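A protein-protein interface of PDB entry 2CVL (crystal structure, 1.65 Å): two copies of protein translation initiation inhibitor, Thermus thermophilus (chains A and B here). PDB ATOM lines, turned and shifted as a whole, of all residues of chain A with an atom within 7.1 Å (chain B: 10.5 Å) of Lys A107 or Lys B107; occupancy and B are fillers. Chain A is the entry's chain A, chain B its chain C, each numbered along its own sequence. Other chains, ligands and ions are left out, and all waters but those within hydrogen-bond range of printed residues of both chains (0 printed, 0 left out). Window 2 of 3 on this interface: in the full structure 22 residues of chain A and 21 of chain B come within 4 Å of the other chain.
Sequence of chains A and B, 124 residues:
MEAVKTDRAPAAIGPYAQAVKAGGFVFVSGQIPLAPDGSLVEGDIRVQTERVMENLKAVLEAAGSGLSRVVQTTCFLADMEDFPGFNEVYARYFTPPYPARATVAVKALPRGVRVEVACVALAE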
ATOM      1  N   LEU A  77      13.167   2.405 -33.839  1.00  0.00           N
ATOM      2  CA  LEU A  77      13.345   3.839 -34.050  1.00  0.00           C
ATOM      3  C   LEU A  77      13.444   4.553 -32.712  1.00  0.00           C
ATOM      4  O   LEU A  77      12.781   4.170 -31.749  1.00  0.00           O
ATOM      5  CB  LEU A  77      12.159   4.417 -34.828  1.00  0.00           C
ATOM      6  CG  LEU A  77      11.932   3.906 -36.251  1.00  0.00           C
ATOM      7  CD1 LEU A  77      10.631   4.473 -36.793  1.00  0.00           C
ATOM      8  CD2 LEU A  77      13.099   4.312 -37.128  1.00  0.00           C
ATOM      9  N   ALA A  78      14.264   5.598 -32.659  1.00  0.00           N
ATOM     10  CA  ALA A  78      14.432   6.361 -31.427  1.00  0.00           C
ATOM     11  C   ALA A  78      13.359   7.442 -31.291  1.00  0.00           C
ATOM     12  O   ALA A  78      13.125   7.956 -30.197  1.00  0.00           O
ATOM     13  CB  ALA A  78      15.814   6.994 -31.392  1.00  0.00           C
ATOM     14  N   ASP A  79      12.710   7.781 -32.401  1.00  0.00           N
ATOM     15  CA  ASP A  79      11.667   8.806 -32.400  1.00  0.00           C
ATOM     16  C   ASP A  79      10.555   8.357 -33.342  1.00  0.00           C
ATOM     17  O   ASP A  79      10.771   8.238 -34.545  1.00  0.00           O
ATOM     18  CB  ASP A  79      12.243  10.140 -32.890  1.00  0.00           C
ATOM     19  CG  ASP A  79      11.309  11.316 -32.640  1.00  0.00           C
ATOM     20  OD1 ASP A  79      10.074  11.130 -32.651  1.00  0.00           O
ATOM     21  OD2 ASP A  79      11.819  12.440 -32.448  1.00  0.00           O
ATOM     22  N   MET A  80       9.367   8.113 -32.802  1.00  0.00           N
ATOM     23  CA  MET A  80       8.257   7.667 -33.632  1.00  0.00           C
ATOM     24  C   MET A  80       7.904   8.680 -34.717  1.00  0.00           C
ATOM     25  O   MET A  80       7.299   8.326 -35.729  1.00  0.00           O
ATOM     26  CB  MET A  80       7.029   7.368 -32.771  1.00  0.00           C
ATOM     27  CG  MET A  80       5.884   6.743 -33.547  1.00  0.00           C
ATOM     28  SD  MET A  80       5.052   5.281 -32.597  1.00  0.00           S
ATOM     29  CE  MET A  80       3.792   6.293 -31.548  1.00  0.00           C
ATOM     30  N   VAL A 104       9.075  -0.786 -33.625  1.00  0.00           N
ATOM     31  CA  VAL A 104       8.824  -0.231 -32.297  1.00  0.00           C
ATOM     32  C   VAL A 104       9.724   0.973 -32.074  1.00  0.00           C
ATOM     33  O   VAL A 104      10.705   1.165 -32.791  1.00  0.00           O
ATOM     34  CB  VAL A 104       9.115  -1.244 -31.174  1.00  0.00           C
ATOM     35  CG1 VAL A 104       8.309  -2.508 -31.388  1.00  0.00           C
ATOM     36  CG2 VAL A 104      10.598  -1.538 -31.118  1.00  0.00           C
ATOM     37  N   ALA A 105       9.380   1.783 -31.078  1.00  0.00           N
ATOM     38  CA  ALA A 105      10.168   2.960 -30.744  1.00  0.00           C
ATOM     39  C   ALA A 105      10.808   2.755 -29.376  1.00  0.00           C
ATOM     40  O   ALA A 105      10.157   2.302 -28.433  1.00  0.00           O
ATOM     41  CB  ALA A 105       9.278   4.203 -30.730  1.00  0.00           C
ATOM     42  N   VAL A 106      12.095   3.068 -29.279  1.00  0.00           N
ATOM     43  CA  VAL A 106      12.812   2.939 -28.020  1.00  0.00           C
ATOM     44  C   VAL A 106      13.309   4.315 -27.597  1.00  0.00           C
ATOM     45  O   VAL A 106      13.376   5.234 -28.415  1.00  0.00           O
ATOM     46  CB  VAL A 106      14.001   1.975 -28.151  1.00  0.00           C
ATOM     47  CG1 VAL A 106      13.491   0.557 -28.341  1.00  0.00           C
ATOM     48  CG2 VAL A 106      14.884   2.393 -29.326  1.00  0.00           C
ATOM     49  N   LYS A 107      13.637   4.466 -26.318  1.00  0.00           N
ATOM     50  CA  LYS A 107      14.109   5.749 -25.808  1.00  0.00           C
ATOM     51  C   LYS A 107      15.375   6.247 -26.489  1.00  0.00           C
ATOM     52  O   LYS A 107      15.506   7.438 -26.772  1.00  0.00           O
ATOM     53  CB  LYS A 107      14.346   5.675 -24.296  1.00  0.00           C
ATOM     54  CG  LYS A 107      13.076   5.667 -23.467  1.00  0.00           C
ATOM     55  CD  LYS A 107      13.389   5.831 -21.988  1.00  0.00           C
ATOM     56  CE  LYS A 107      12.116   5.927 -21.162  1.00  0.00           C
ATOM     57  NZ  LYS A 107      12.406   6.170 -19.721  1.00  0.00           N
ATOM     58  N   ALA A 108      16.313   5.340 -26.736  1.00  0.00           N
ATOM     59  CA  ALA A 108      17.564   5.709 -27.383  1.00  0.00           C
ATOM     60  C   ALA A 108      18.278   4.493 -27.960  1.00  0.00           C
ATOM     61  O   ALA A 108      18.141   3.376 -27.461  1.00  0.00           O
ATOM     62  CB  ALA A 108      18.472   6.431 -26.393  1.00  0.00           C
ATOM     63  N   LEU A 109      19.037   4.727 -29.024  1.00  0.00           N
ATOM     64  CA  LEU A 109      19.791   3.679 -29.689  1.00  0.00           C
ATOM     65  C   LEU A 109      21.275   4.009 -29.576  1.00  0.00           C
ATOM     66  O   LEU A 109      21.639   5.120 -29.192  1.00  0.00           O
ATOM     67  CB  LEU A 109      19.372   3.593 -31.160  1.00  0.00           C
ATOM     68  CG  LEU A 109      17.999   2.969 -31.438  1.00  0.00           C
ATOM     69  CD1 LEU A 109      17.580   3.244 -32.873  1.00  0.00           C
ATOM     70  CD2 LEU A 109      18.062   1.471 -31.177  1.00  0.00           C
ATOM     71  N   PHE B  76       5.558  -7.035 -27.845  1.00  0.00           N
ATOM     72  CA  PHE B  76       5.978  -5.745 -27.316  1.00  0.00           C
ATOM     73  C   PHE B  76       4.823  -5.071 -26.598  1.00  0.00           C
ATOM     74  O   PHE B  76       3.702  -5.019 -27.107  1.00  0.00           O
ATOM     75  CB  PHE B  76       6.462  -4.811 -28.430  1.00  0.00           C
ATOM     76  CG  PHE B  76       7.596  -5.360 -29.238  1.00  0.00           C
ATOM     77  CD1 PHE B  76       7.351  -6.057 -30.416  1.00  0.00           C
ATOM     78  CD2 PHE B  76       8.911  -5.168 -28.834  1.00  0.00           C
ATOM     79  CE1 PHE B  76       8.403  -6.556 -31.183  1.00  0.00           C
ATOM     80  CE2 PHE B  76       9.970  -5.662 -29.592  1.00  0.00           C
ATOM     81  CZ  PHE B  76       9.713  -6.357 -30.771  1.00  0.00           C
ATOM     82  N   LEU B  77       5.102  -4.566 -25.405  1.00  0.00           N
ATOM     83  CA  LEU B  77       4.103  -3.862 -24.620  1.00  0.00           C
ATOM     84  C   LEU B  77       4.655  -2.470 -24.367  1.00  0.00           C
ATOM     85  O   LEU B  77       5.863  -2.251 -24.461  1.00  0.00           O
ATOM     86  CB  LEU B  77       3.861  -4.567 -23.284  1.00  0.00           C
ATOM     87  CG  LEU B  77       3.294  -5.985 -23.363  1.00  0.00           C
ATOM     88  CD1 LEU B  77       3.176  -6.571 -21.961  1.00  0.00           C
ATOM     89  CD2 LEU B  77       1.936  -5.951 -24.041  1.00  0.00           C
ATOM     90  N   ALA B  78       3.766  -1.531 -24.071  1.00  0.00           N
ATOM     91  CA  ALA B  78       4.189  -0.168 -23.787  1.00  0.00           C
ATOM     92  C   ALA B  78       4.225   0.068 -22.278  1.00  0.00           C
ATOM     93  O   ALA B  78       4.814   1.042 -21.813  1.00  0.00           O
ATOM     94  CB  ALA B  78       3.242   0.824 -24.453  1.00  0.00           C
ATOM     95  N   ASP B  79       3.605  -0.831 -21.517  1.00  0.00           N
ATOM     96  CA  ASP B  79       3.557  -0.706 -20.056  1.00  0.00           C
ATOM     97  C   ASP B  79       3.779  -2.060 -19.387  1.00  0.00           C
ATOM     98  O   ASP B  79       3.074  -3.022 -19.685  1.00  0.00           O
ATOM     99  CB  ASP B  79       2.192  -0.156 -19.632  1.00  0.00           C
ATOM    100  CG  ASP B  79       2.163   0.295 -18.183  1.00  0.00           C
ATOM    101  OD1 ASP B  79       2.876  -0.298 -17.345  1.00  0.00           O
ATOM    102  OD2 ASP B  79       1.410   1.244 -17.879  1.00  0.00           O
ATOM    103  N   MET B  80       4.749  -2.133 -18.477  1.00  0.00           N
ATOM    104  CA  MET B  80       5.046  -3.381 -17.775  1.00  0.00           C
ATOM    105  C   MET B  80       3.838  -3.854 -16.969  1.00  0.00           C
ATOM    106  O   MET B  80       3.662  -5.049 -16.733  1.00  0.00           O
ATOM    107  CB  MET B  80       6.242  -3.197 -16.831  1.00  0.00           C
ATOM    108  CG  MET B  80       5.999  -2.201 -15.696  1.00  0.00           C
ATOM    109  SD  MET B  80       7.435  -2.128 -14.387  1.00  0.00           S
ATOM    110  CE  MET B  80       6.860  -3.572 -13.238  1.00  0.00           C
ATOM    111  N   ASP B  82       0.886  -3.972 -17.897  1.00  0.00           N
ATOM    112  CA  ASP B  82      -0.094  -4.639 -18.750  1.00  0.00           C
ATOM    113  C   ASP B  82       0.207  -6.121 -18.987  1.00  0.00           C
ATOM    114  O   ASP B  82      -0.590  -6.813 -19.617  1.00  0.00           O
ATOM    115  CB  ASP B  82      -0.210  -3.933 -20.107  1.00  0.00           C
ATOM    116  CG  ASP B  82      -1.089  -2.694 -20.054  1.00  0.00           C
ATOM    117  OD1 ASP B  82      -1.904  -2.571 -19.113  1.00  0.00           O
ATOM    118  OD2 ASP B  82      -0.976  -1.852 -20.970  1.00  0.00           O
ATOM    119  N   VAL B 104       8.810  -7.878 -24.083  1.00  0.00           N
ATOM    120  CA  VAL B 104       9.499  -6.726 -23.512  1.00  0.00           C
ATOM    121  C   VAL B 104       8.571  -5.527 -23.533  1.00  0.00           C
ATOM    122  O   VAL B 104       7.566  -5.524 -24.243  1.00  0.00           O
ATOM    123  CB  VAL B 104      10.762  -6.330 -24.314  1.00  0.00           C
ATOM    124  CG1 VAL B 104      11.717  -7.501 -24.416  1.00  0.00           C
ATOM    125  CG2 VAL B 104      10.364  -5.831 -25.700  1.00  0.00           C
ATOM    126  N   ALA B 105       8.908  -4.516 -22.739  1.00  0.00           N
ATOM    127  CA  ALA B 105       8.134  -3.284 -22.715  1.00  0.00           C
ATOM    128  C   ALA B 105       9.046  -2.242 -23.352  1.00  0.00           C
ATOM    129  O   ALA B 105      10.246  -2.194 -23.054  1.00  0.00           O
ATOM    130  CB  ALA B 105       7.790  -2.888 -21.280  1.00  0.00           C
ATOM    131  N   VAL B 106       8.489  -1.427 -24.240  1.00  0.00           N
ATOM    132  CA  VAL B 106       9.265  -0.395 -24.920  1.00  0.00           C
ATOM    133  C   VAL B 106       8.631   0.979 -24.745  1.00  0.00           C
ATOM    134  O   VAL B 106       7.517   1.098 -24.237  1.00  0.00           O
ATOM    135  CB  VAL B 106       9.401  -0.699 -26.434  1.00  0.00           C
ATOM    136  CG1 VAL B 106      10.208  -1.970 -26.636  1.00  0.00           C
ATOM    137  CG2 VAL B 106       8.022  -0.843 -27.074  1.00  0.00           C
ATOM    138  N   LYS B 107       9.347   2.014 -25.173  1.00  0.00           N
ATOM    139  CA  LYS B 107       8.855   3.381 -25.047  1.00  0.00           C
ATOM    140  C   LYS B 107       7.500   3.585 -25.720  1.00  0.00           C
ATOM    141  O   LYS B 107       6.553   4.053 -25.091  1.00  0.00           O
ATOM    142  CB  LYS B 107       9.859   4.365 -25.648  1.00  0.00           C
ATOM    143  CG  LYS B 107       9.480   5.825 -25.454  1.00  0.00           C
ATOM    144  CD  LYS B 107      10.440   6.753 -26.189  1.00  0.00           C
ATOM    145  CE  LYS B 107      10.313   6.591 -27.696  1.00  0.00           C
ATOM    146  NZ  LYS B 107      11.235   7.490 -28.431  1.00  0.00           N
ATOM    147  N   ALA B 108       7.412   3.232 -26.997  1.00  0.00           N
ATOM    148  CA  ALA B 108       6.165   3.422 -27.725  1.00  0.00           C
ATOM    149  C   ALA B 108       5.998   2.452 -28.876  1.00  0.00           C
ATOM    150  O   ALA B 108       6.964   1.869 -29.368  1.00  0.00           O
ATOM    151  CB  ALA B 108       6.084   4.855 -28.244  1.00  0.00           C
ATOM    152  N   LEU B 109       4.753   2.304 -29.309  1.00  0.00           N
ATOM    153  CA  LEU B 109       4.410   1.405 -30.397  1.00  0.00           C
ATOM    154  C   LEU B 109       3.637   2.178 -31.454  1.00  0.00           C
ATOM    155  O   LEU B 109       3.202   3.302 -31.211  1.00  0.00           O
ATOM    156  CB  LEU B 109       3.558   0.259 -29.856  1.00  0.00           C
ATOM    157  CG  LEU B 109       4.290  -0.622 -28.843  1.00  0.00           C
ATOM    158  CD1 LEU B 109       3.298  -1.534 -28.136  1.00  0.00           C
ATOM    159  CD2 LEU B 109       5.357  -1.437 -29.565  1.00  0.00           C
ATOM    160  N   PRO B 110       3.464   1.589 -32.646  1.00  0.00           N
ATOM    161  CA  PRO B 110       2.726   2.277 -33.706  1.00  0.00           C
ATOM    162  C   PRO B 110       1.391   2.838 -33.221  1.00  0.00           C
ATOM    163  O   PRO B 110       0.628   2.151 -32.542  1.00  0.00           O
ATOM    164  CB  PRO B 110       2.550   1.186 -34.755  1.00  0.00           C
ATOM    165  CG  PRO B 110       3.817   0.397 -34.613  1.00  0.00           C
ATOM    166  CD  PRO B 110       3.956   0.280 -33.112  1.00  0.00           C
ATOM    167  N   ARG B 111       1.127   4.096 -33.565  1.00  0.00           N
ATOM    168  CA  ARG B 111      -0.114   4.775 -33.203  1.00  0.00           C
ATOM    169  C   ARG B 111      -0.419   4.859 -31.706  1.00  0.00           C
ATOM    170  O   ARG B 111      -1.560   5.111 -31.308  1.00  0.00           O
ATOM    171  CB  ARG B 111      -1.276   4.121 -33.955  1.00  0.00           C
ATOM    172  CG  ARG B 111      -1.005   4.054 -35.455  1.00  0.00           C
ATOM    173  CD  ARG B 111      -2.212   3.616 -36.250  1.00  0.00           C
ATOM    174  NE  ARG B 111      -3.341   4.521 -36.061  1.00  0.00           N
ATOM    175  CZ  ARG B 111      -4.425   4.522 -36.826  1.00  0.00           C
ATOM    176  NH1 ARG B 111      -4.521   3.669 -37.837  1.00  0.00           N
ATOM    177  NH2 ARG B 111      -5.416   5.367 -36.574  1.00  0.00           N
ATOM    178  N   GLY B 112       0.605   4.660 -30.883  1.00  0.00           N
ATOM    179  CA  GLY B 112       0.431   4.743 -29.442  1.00  0.00           C
ATOM    180  C   GLY B 112      -0.342   3.613 -28.782  1.00  0.00           C
ATOM    181  O   GLY B 112      -0.877   3.785 -27.692  1.00  0.00           O
ATOM    182  N   VAL B 113      -0.390   2.452 -29.425  1.00  0.00           N
ATOM    183  CA  VAL B 113      -1.113   1.311 -28.872  1.00  0.00           C
ATOM    184  C   VAL B 113      -0.379   0.678 -27.697  1.00  0.00           C
ATOM    185  O   VAL B 113       0.808   0.935 -27.476  1.00  0.00           O
ATOM    186  CB  VAL B 113      -1.362   0.230 -29.950  1.00  0.00           C
ATOM    187  CG1 VAL B 113      -2.117   0.841 -31.123  1.00  0.00           C
ATOM    188  CG2 VAL B 113      -0.037  -0.365 -30.421  1.00  0.00           C
ATOM    189  N   ARG B 114      -1.094  -0.157 -26.952  1.00  0.00           N
ATOM    190  CA  ARG B 114      -0.543  -0.833 -25.782  1.00  0.00           C
ATOM    191  C   ARG B 114       0.207  -2.108 -26.105  1.00  0.00           C
ATOM    192  O   ARG B 114       0.988  -2.594 -25.285  1.00  0.00           O
ATOM    193  CB  ARG B 114      -1.660  -1.221 -24.813  1.00  0.00           C
ATOM    194  CG  ARG B 114      -2.301  -0.087 -24.055  1.00  0.00           C
ATOM    195  CD  ARG B 114      -3.464  -0.622 -23.225  1.00  0.00           C
ATOM    196  NE  ARG B 114      -4.123   0.447 -22.484  1.00  0.00           N
ATOM    197  CZ  ARG B 114      -3.605   1.043 -21.419  1.00  0.00           C
ATOM    198  NH1 ARG B 114      -2.419   0.672 -20.956  1.00  0.00           N
ATOM    199  NH2 ARG B 114      -4.264   2.030 -20.826  1.00  0.00           N
ATOM    200  N   VAL B 115      -0.023  -2.652 -27.293  1.00  0.00           N
ATOM    201  CA  VAL B 115       0.587  -3.928 -27.619  1.00  0.00           C
ATOM    202  C   VAL B 115       0.760  -4.195 -29.105  1.00  0.00           C
ATOM    203  O   VAL B 115      -0.063  -3.788 -29.926  1.00  0.00           O
ATOM    204  CB  VAL B 115      -0.280  -5.052 -26.994  1.00  0.00           C
ATOM    205  CG1 VAL B 115      -1.735  -4.866 -27.414  1.00  0.00           C
ATOM    206  CG2 VAL B 115       0.211  -6.424 -27.418  1.00  0.00           C
ATOM    207  N   GLU B 116       1.855  -4.875 -29.435  1.00  0.00           N
ATOM    208  CA  GLU B 116       2.154  -5.276 -30.805  1.00  0.00           C
ATOM    209  C   GLU B 116       2.728  -6.682 -30.740  1.00  0.00           C
ATOM    210  O   GLU B 116       3.643  -6.945 -29.961  1.00  0.00           O
ATOM    211  CB  GLU B 116       3.184  -4.351 -31.454  1.00  0.00           C
ATOM    212  CG  GLU B 116       3.498  -4.734 -32.903  1.00  0.00           C
ATOM    213  CD  GLU B 116       4.583  -3.872 -33.524  1.00  0.00           C
ATOM    214  OE1 GLU B 116       4.804  -2.739 -33.038  1.00  0.00           O
ATOM    215  OE2 GLU B 116       5.206  -4.321 -34.511  1.00  0.00           O
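O of Ala A78 is in hydrogen-bond range of NZ of Lys B107 (2.6 Å).
O of Ala A105 is in hydrogen-bond range of N of Lys B107.
The backbone NH (N) of Ala A105 sits at hydrogen-bond distance from the backbone carbonyl oxygen (O) of Ala B108 (3.0 Å).
The backbone carbonyl oxygen (O) of Val A106 is in hydrogen-bond range of the side-chain amino group (NZ) of Lys B107, at 3.1 Å.
SD of Met A80 sits close to O of Leu B109, 3.0 Å away.
Ala A78 touches Lys B107, but with the chains exchanged Lys A107 does not touch Ala B78 (8.8 Å).
Met A80 touches Leu B109, but with the chains exchanged Leu A109 does not touch Met B80 (18.7 Å).
Val A104 touches Leu B109, but with the chains exchanged Leu A109 does not touch Val B104 (11.9 Å).
Ala A105 touches Lys B107, but with the chains exchanged Lys A107 does not touch Ala B105 (8.2 Å).
Of the 14 pairs that touch across the chains among the printed residues, 1 has its exchanged pair printed and touching as well.
The backbone NH (N) of Leu A77 lies within hydrogen-bond range of the backbone carbonyl oxygen (O) of Val A104, at 2.9 Å.
O of Leu A77 lies within hydrogen-bond range of N of Val A106.
N of Phe B76 is in hydrogen-bond range of O of Glu B116 (2.9 Å).
The backbone carbonyl oxygen (O) of Leu B77 is in hydrogen-bond range of the backbone NH (N) of Val B106 (2.8 Å).
Hydrophobic or aromatic side chains of chain B that line the printed part of chain A: Phe B76, Val B106 and Leu B109.
Among the printed residues, no Asp or Glu carboxylate lies within 4 Å of a Lys or Arg side-chain nitrogen of the other chain.
Among the printed residues, merely in contact across the chains: Val A104 with Leu B109 (3.6 Å), Val A104 with Phe B76 (3.6 Å), Met A80 with Gly B112 (3.6 Å), Ala A105 with Val B106 (3.7 Å), Lys A107 with Lys B107 (3.8 Å), Val A104 with Glu B116 (3.9 Å), Met A80 with Pro B110 (3.96 Å), Val A104 with Ala B108 (3.97 Å) and Met A80 with Arg B111 (3.9997 Å).
Printed residues of chain B within 4 Å of Lys A107: Lys B107.
Lys B107 touches just these residues of chain A: Ala A78, Ala A105, Val A106 and Lys A107.
Ala A78 touches just one residue of chain B: Lys B107 (2.6 Å).
No residue of chain B comes within 4 Å of Asp A79.
Ala A105 touches just these residues of chain B: Val B106, Lys B107 and Ala B108.
Val A106 touches just one residue of chain B: Lys B107.
No residue of chain B comes within 4 Å of Ala A108.
Of the printed residues of chain A, Phe B76 touches Val A104.
Of the printed residues of chain B, Val A104 touches Phe B76 (3.6 Å), Ala B108 (3.97 Å), Leu B109 (3.6 Å) and Glu B116 (3.9 Å).
Of the printed residues of chain A, Ala B108 touches Val A104 (3.97 Å) and Ala A105 (3.0 Å).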
